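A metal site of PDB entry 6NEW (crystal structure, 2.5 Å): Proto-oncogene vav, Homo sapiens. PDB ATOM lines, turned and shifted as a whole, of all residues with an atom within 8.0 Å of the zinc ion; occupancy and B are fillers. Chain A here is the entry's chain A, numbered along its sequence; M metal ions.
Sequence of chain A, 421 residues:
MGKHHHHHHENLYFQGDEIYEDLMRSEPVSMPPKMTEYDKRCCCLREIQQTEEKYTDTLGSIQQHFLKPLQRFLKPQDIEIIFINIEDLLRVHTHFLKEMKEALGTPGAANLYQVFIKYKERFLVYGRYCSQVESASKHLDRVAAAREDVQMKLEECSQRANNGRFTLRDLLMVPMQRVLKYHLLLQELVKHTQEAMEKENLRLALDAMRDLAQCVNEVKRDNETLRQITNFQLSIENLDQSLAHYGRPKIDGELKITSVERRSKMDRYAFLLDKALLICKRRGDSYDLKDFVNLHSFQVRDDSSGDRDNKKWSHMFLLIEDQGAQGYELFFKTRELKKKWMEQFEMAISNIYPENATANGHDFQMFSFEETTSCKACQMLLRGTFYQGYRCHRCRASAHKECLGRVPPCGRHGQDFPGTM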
ATOM      1  N   SER A 374      -7.006 -13.535  -8.974  1.00  0.00           N
ATOM      2  CA  SER A 374      -8.420 -13.653  -9.285  1.00  0.00           C
ATOM      3  C   SER A 374      -9.244 -13.455  -8.008  1.00  0.00           C
ATOM      4  O   SER A 374      -8.749 -13.680  -6.888  1.00  0.00           O
ATOM      5  CB  SER A 374      -8.730 -14.999  -9.947  1.00  0.00           C
ATOM      6  OG  SER A 374      -8.322 -16.073  -9.122  1.00  0.00           O
ATOM      7  N   CYS A 375     -10.485 -12.984  -8.175  1.00  0.00           N
ATOM      8  CA  CYS A 375     -11.431 -12.715  -7.102  1.00  0.00           C
ATOM      9  C   CYS A 375     -11.931 -14.022  -6.498  1.00  0.00           C
ATOM     10  O   CYS A 375     -12.352 -14.899  -7.230  1.00  0.00           O
ATOM     11  CB  CYS A 375     -12.581 -11.863  -7.633  1.00  0.00           C
ATOM     12  SG  CYS A 375     -13.915 -11.637  -6.447  1.00  0.00           S
ATOM     13  N   LYS A 376     -11.893 -14.157  -5.153  1.00  0.00           N
ATOM     14  CA  LYS A 376     -12.352 -15.368  -4.459  1.00  0.00           C
ATOM     15  C   LYS A 376     -13.867 -15.597  -4.545  1.00  0.00           C
ATOM     16  O   LYS A 376     -14.324 -16.688  -4.216  1.00  0.00           O
ATOM     17  CB  LYS A 376     -11.896 -15.385  -2.995  1.00  0.00           C
ATOM     18  CG  LYS A 376     -10.390 -15.522  -2.846  1.00  0.00           C
ATOM     19  CD  LYS A 376     -10.009 -16.956  -2.595  1.00  0.00           C
ATOM     20  CE  LYS A 376      -8.715 -17.253  -3.292  1.00  0.00           C
ATOM     21  NZ  LYS A 376      -7.564 -16.676  -2.559  1.00  0.00           N
ATOM     22  N   ALA A 377     -14.625 -14.586  -5.017  1.00  0.00           N
ATOM     23  CA  ALA A 377     -16.063 -14.699  -5.179  1.00  0.00           C
ATOM     24  C   ALA A 377     -16.509 -15.024  -6.619  1.00  0.00           C
ATOM     25  O   ALA A 377     -17.200 -16.027  -6.809  1.00  0.00           O
ATOM     26  CB  ALA A 377     -16.747 -13.443  -4.697  1.00  0.00           C
ATOM     27  N   CYS A 378     -16.136 -14.189  -7.608  1.00  0.00           N
ATOM     28  CA  CYS A 378     -16.542 -14.349  -9.000  1.00  0.00           C
ATOM     29  C   CYS A 378     -15.546 -15.121  -9.884  1.00  0.00           C
ATOM     30  O   CYS A 378     -15.905 -15.531 -10.977  1.00  0.00           O
ATOM     31  CB  CYS A 378     -16.884 -12.995  -9.624  1.00  0.00           C
ATOM     32  SG  CYS A 378     -15.446 -11.920  -9.832  1.00  0.00           S
ATOM     33  N   GLN A 379     -14.301 -15.330  -9.393  1.00  0.00           N
ATOM     34  CA  GLN A 379     -13.212 -16.042 -10.092  1.00  0.00           C
ATOM     35  C   GLN A 379     -12.652 -15.254 -11.282  1.00  0.00           C
ATOM     36  O   GLN A 379     -11.779 -15.761 -12.001  1.00  0.00           O
ATOM     37  CB  GLN A 379     -13.586 -17.492 -10.492  1.00  0.00           C
ATOM     38  CG  GLN A 379     -14.449 -18.296  -9.489  1.00  0.00           C
ATOM     39  CD  GLN A 379     -13.834 -18.480  -8.112  1.00  0.00           C
ATOM     40  OE1 GLN A 379     -12.638 -18.739  -7.954  1.00  0.00           O
ATOM     41  NE2 GLN A 379     -14.669 -18.369  -7.090  1.00  0.00           N
ATOM     42  N   MET A 380     -13.126 -13.998 -11.487  1.00  0.00           N
ATOM     43  CA  MET A 380     -12.598 -13.127 -12.523  1.00  0.00           C
ATOM     44  C   MET A 380     -11.370 -12.392 -11.964  1.00  0.00           C
ATOM     45  O   MET A 380     -11.215 -12.250 -10.756  1.00  0.00           O
ATOM     46  CB  MET A 380     -13.638 -12.126 -13.059  1.00  0.00           C
ATOM     47  CG  MET A 380     -14.841 -12.791 -13.750  1.00  0.00           C
ATOM     48  SD  MET A 380     -14.415 -14.011 -15.024  1.00  0.00           S
ATOM     49  CE  MET A 380     -15.737 -15.197 -14.750  1.00  0.00           C
ATOM     50  N   LEU A 381     -10.477 -11.993 -12.861  1.00  0.00           N
ATOM     51  CA  LEU A 381      -9.222 -11.322 -12.548  1.00  0.00           C
ATOM     52  C   LEU A 381      -9.407 -10.003 -11.831  1.00  0.00           C
ATOM     53  O   LEU A 381     -10.335  -9.266 -12.134  1.00  0.00           O
ATOM     54  CB  LEU A 381      -8.457 -11.026 -13.853  1.00  0.00           C
ATOM     55  CG  LEU A 381      -7.772 -12.171 -14.560  1.00  0.00           C
ATOM     56  CD1 LEU A 381      -7.400 -11.776 -15.966  1.00  0.00           C
ATOM     57  CD2 LEU A 381      -6.542 -12.584 -13.816  1.00  0.00           C
ATOM     58  N   LEU A 382      -8.438  -9.664 -10.947  1.00  0.00           N
ATOM     59  CA  LEU A 382      -8.369  -8.358 -10.330  1.00  0.00           C
ATOM     60  C   LEU A 382      -7.654  -7.486 -11.366  1.00  0.00           C
ATOM     61  O   LEU A 382      -6.580  -7.838 -11.840  1.00  0.00           O
ATOM     62  CB  LEU A 382      -7.678  -8.404  -8.966  1.00  0.00           C
ATOM     63  CG  LEU A 382      -8.671  -8.645  -7.850  1.00  0.00           C
ATOM     64  CD1 LEU A 382      -8.090  -9.427  -6.742  1.00  0.00           C
ATOM     65  CD2 LEU A 382      -9.213  -7.359  -7.318  1.00  0.00           C
ATOM     66  N   ARG A 383      -8.335  -6.428 -11.821  1.00  0.00           N
ATOM     67  CA  ARG A 383      -7.942  -5.574 -12.941  1.00  0.00           C
ATOM     68  C   ARG A 383      -7.054  -4.381 -12.647  1.00  0.00           C
ATOM     69  O   ARG A 383      -7.373  -3.566 -11.776  1.00  0.00           O
ATOM     70  CB  ARG A 383      -9.207  -5.060 -13.642  1.00  0.00           C
ATOM     71  CG  ARG A 383      -9.987  -6.147 -14.340  1.00  0.00           C
ATOM     72  CD  ARG A 383     -11.439  -6.048 -13.988  1.00  0.00           C
ATOM     73  NE  ARG A 383     -12.132  -7.304 -14.235  1.00  0.00           N
ATOM     74  CZ  ARG A 383     -13.351  -7.569 -13.793  1.00  0.00           C
ATOM     75  NH1 ARG A 383     -14.019  -6.677 -13.079  1.00  0.00           N
ATOM     76  NH2 ARG A 383     -13.913  -8.744 -14.055  1.00  0.00           N
ATOM     77  N   SER A 398      -8.382 -12.533  -1.744  1.00  0.00           N
ATOM     78  CA  SER A 398      -8.351 -11.396  -2.633  1.00  0.00           C
ATOM     79  C   SER A 398      -9.745 -11.274  -3.250  1.00  0.00           C
ATOM     80  O   SER A 398     -10.381 -12.296  -3.459  1.00  0.00           O
ATOM     81  CB  SER A 398      -7.300 -11.643  -3.711  1.00  0.00           C
ATOM     82  OG  SER A 398      -7.638 -12.812  -4.450  1.00  0.00           O
ATOM     83  N   ALA A 399     -10.230 -10.041  -3.536  1.00  0.00           N
ATOM     84  CA  ALA A 399     -11.579  -9.794  -4.092  1.00  0.00           C
ATOM     85  C   ALA A 399     -11.760  -8.393  -4.665  1.00  0.00           C
ATOM     86  O   ALA A 399     -11.054  -7.461  -4.267  1.00  0.00           O
ATOM     87  CB  ALA A 399     -12.635 -10.034  -3.014  1.00  0.00           C
ATOM     88  N   HIS A 400     -12.746  -8.230  -5.573  1.00  0.00           N
ATOM     89  CA  HIS A 400     -13.109  -6.908  -6.118  1.00  0.00           C
ATOM     90  C   HIS A 400     -13.981  -6.206  -5.063  1.00  0.00           C
ATOM     91  O   HIS A 400     -14.613  -6.900  -4.259  1.00  0.00           O
ATOM     92  CB  HIS A 400     -13.939  -6.994  -7.415  1.00  0.00           C
ATOM     93  CG  HIS A 400     -13.321  -7.730  -8.555  1.00  0.00           C
ATOM     94  ND1 HIS A 400     -13.829  -8.951  -8.976  1.00  0.00           N
ATOM     95  CD2 HIS A 400     -12.340  -7.363  -9.395  1.00  0.00           C
ATOM     96  CE1 HIS A 400     -13.084  -9.314 -10.004  1.00  0.00           C
ATOM     97  NE2 HIS A 400     -12.190  -8.380 -10.305  1.00  0.00           N
ATOM     98  N   LYS A 401     -14.071  -4.858  -5.110  1.00  0.00           N
ATOM     99  CA  LYS A 401     -14.900  -4.072  -4.186  1.00  0.00           C
ATOM    100  C   LYS A 401     -16.371  -4.552  -4.148  1.00  0.00           C
ATOM    101  O   LYS A 401     -16.924  -4.673  -3.049  1.00  0.00           O
ATOM    102  CB  LYS A 401     -14.846  -2.573  -4.547  1.00  0.00           C
ATOM    103  CG  LYS A 401     -15.314  -1.673  -3.397  1.00  0.00           C
ATOM    104  CD  LYS A 401     -15.446  -0.204  -3.799  1.00  0.00           C
ATOM    105  CE  LYS A 401     -15.968   0.633  -2.641  1.00  0.00           C
ATOM    106  NZ  LYS A 401     -16.111   2.067  -3.004  1.00  0.00           N
ATOM    107  N   GLU A 402     -16.967  -4.861  -5.314  1.00  0.00           N
ATOM    108  CA  GLU A 402     -18.362  -5.342  -5.445  1.00  0.00           C
ATOM    109  C   GLU A 402     -18.604  -6.756  -4.864  1.00  0.00           C
ATOM    110  O   GLU A 402     -19.716  -7.052  -4.433  1.00  0.00           O
ATOM    111  CB  GLU A 402     -18.837  -5.333  -6.916  1.00  0.00           C
ATOM    112  CG  GLU A 402     -18.265  -4.241  -7.811  1.00  0.00           C
ATOM    113  CD  GLU A 402     -16.983  -4.661  -8.521  1.00  0.00           C
ATOM    114  OE1 GLU A 402     -17.079  -5.515  -9.435  1.00  0.00           O
ATOM    115  OE2 GLU A 402     -15.909  -4.168  -8.145  1.00  0.00           O
ATOM    116  N   CYS A 403     -17.592  -7.636  -4.909  1.00  0.00           N
ATOM    117  CA  CYS A 403     -17.657  -9.042  -4.519  1.00  0.00           C
ATOM    118  C   CYS A 403     -17.390  -9.374  -3.044  1.00  0.00           C
ATOM    119  O   CYS A 403     -17.375 -10.559  -2.725  1.00  0.00           O
ATOM    120  CB  CYS A 403     -16.718  -9.853  -5.413  1.00  0.00           C
ATOM    121  SG  CYS A 403     -16.908  -9.564  -7.184  1.00  0.00           S
ATOM    122  N   LEU A 404     -17.128  -8.383  -2.177  1.00  0.00           N
ATOM    123  CA  LEU A 404     -16.747  -8.605  -0.775  1.00  0.00           C
ATOM    124  C   LEU A 404     -17.723  -9.468   0.047  1.00  0.00           C
ATOM    125  O   LEU A 404     -17.283 -10.393   0.730  1.00  0.00           O
ATOM    126  CB  LEU A 404     -16.466  -7.280  -0.034  1.00  0.00           C
ATOM    127  CG  LEU A 404     -15.334  -6.389  -0.557  1.00  0.00           C
ATOM    128  CD1 LEU A 404     -15.046  -5.305   0.416  1.00  0.00           C
ATOM    129  CD2 LEU A 404     -14.048  -7.189  -0.815  1.00  0.00           C
ATOM    130  N   ARG A 406     -19.712 -11.661  -1.024  1.00  0.00           N
ATOM    131  CA  ARG A 406     -19.837 -12.985  -1.622  1.00  0.00           C
ATOM    132  C   ARG A 406     -18.619 -13.913  -1.479  1.00  0.00           C
ATOM    133  O   ARG A 406     -18.677 -15.053  -1.957  1.00  0.00           O
ATOM    134  CB  ARG A 406     -20.218 -12.852  -3.110  1.00  0.00           C
ATOM    135  CG  ARG A 406     -21.642 -12.336  -3.370  1.00  0.00           C
ATOM    136  CD  ARG A 406     -21.887 -12.237  -4.861  1.00  0.00           C
ATOM    137  NE  ARG A 406     -21.774 -13.539  -5.525  1.00  0.00           N
ATOM    138  CZ  ARG A 406     -22.740 -14.461  -5.604  1.00  0.00           C
ATOM    139  NH1 ARG A 406     -23.916 -14.248  -5.044  1.00  0.00           N
ATOM    140  NH2 ARG A 406     -22.513 -15.602  -6.238  1.00  0.00           N
ATOM    141  N   VAL A 407     -17.535 -13.452  -0.825  1.00  0.00           N
ATOM    142  CA  VAL A 407     -16.347 -14.281  -0.610  1.00  0.00           C
ATOM    143  C   VAL A 407     -16.691 -15.317   0.491  1.00  0.00           C
ATOM    144  O   VAL A 407     -17.306 -14.940   1.481  1.00  0.00           O
ATOM    145  CB  VAL A 407     -15.091 -13.432  -0.257  1.00  0.00           C
ATOM    146  CG1 VAL A 407     -13.859 -14.301   0.049  1.00  0.00           C
ATOM    147  CG2 VAL A 407     -14.767 -12.440  -1.364  1.00  0.00           C
HETATM  148 ZN    ZN M   1     -15.113 -10.519  -7.988  1.00  0.00          ZN
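N of Met 380 lies close to SG of Cys 378 (3.5 Å).
The side-chain sulfur (SG) of Cys 375 sits close to the backbone NH (N) of Ala 377 (3.4 Å).
NE2 of His 400 lies within hydrogen-bond range of O of Leu 381, 2.8 Å away.
N of Cys 375 lies within hydrogen-bond range of O of Met 380, at 2.8 Å.
Within 4 Å of the zinc ion: Cys 375, Cys 378, His 400 and Cys 403.
SG of Cys 403 is bound to the zinc ion, at 2.2 Å.
The zinc ion is bound by the side-chain sulfur (SG) of Cys 375 (2.2 Å).
The zinc ion is bound by ND1 of His 400, 2.3 Å away.
SG of Cys 378 binds the zinc ion (2.3 Å).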
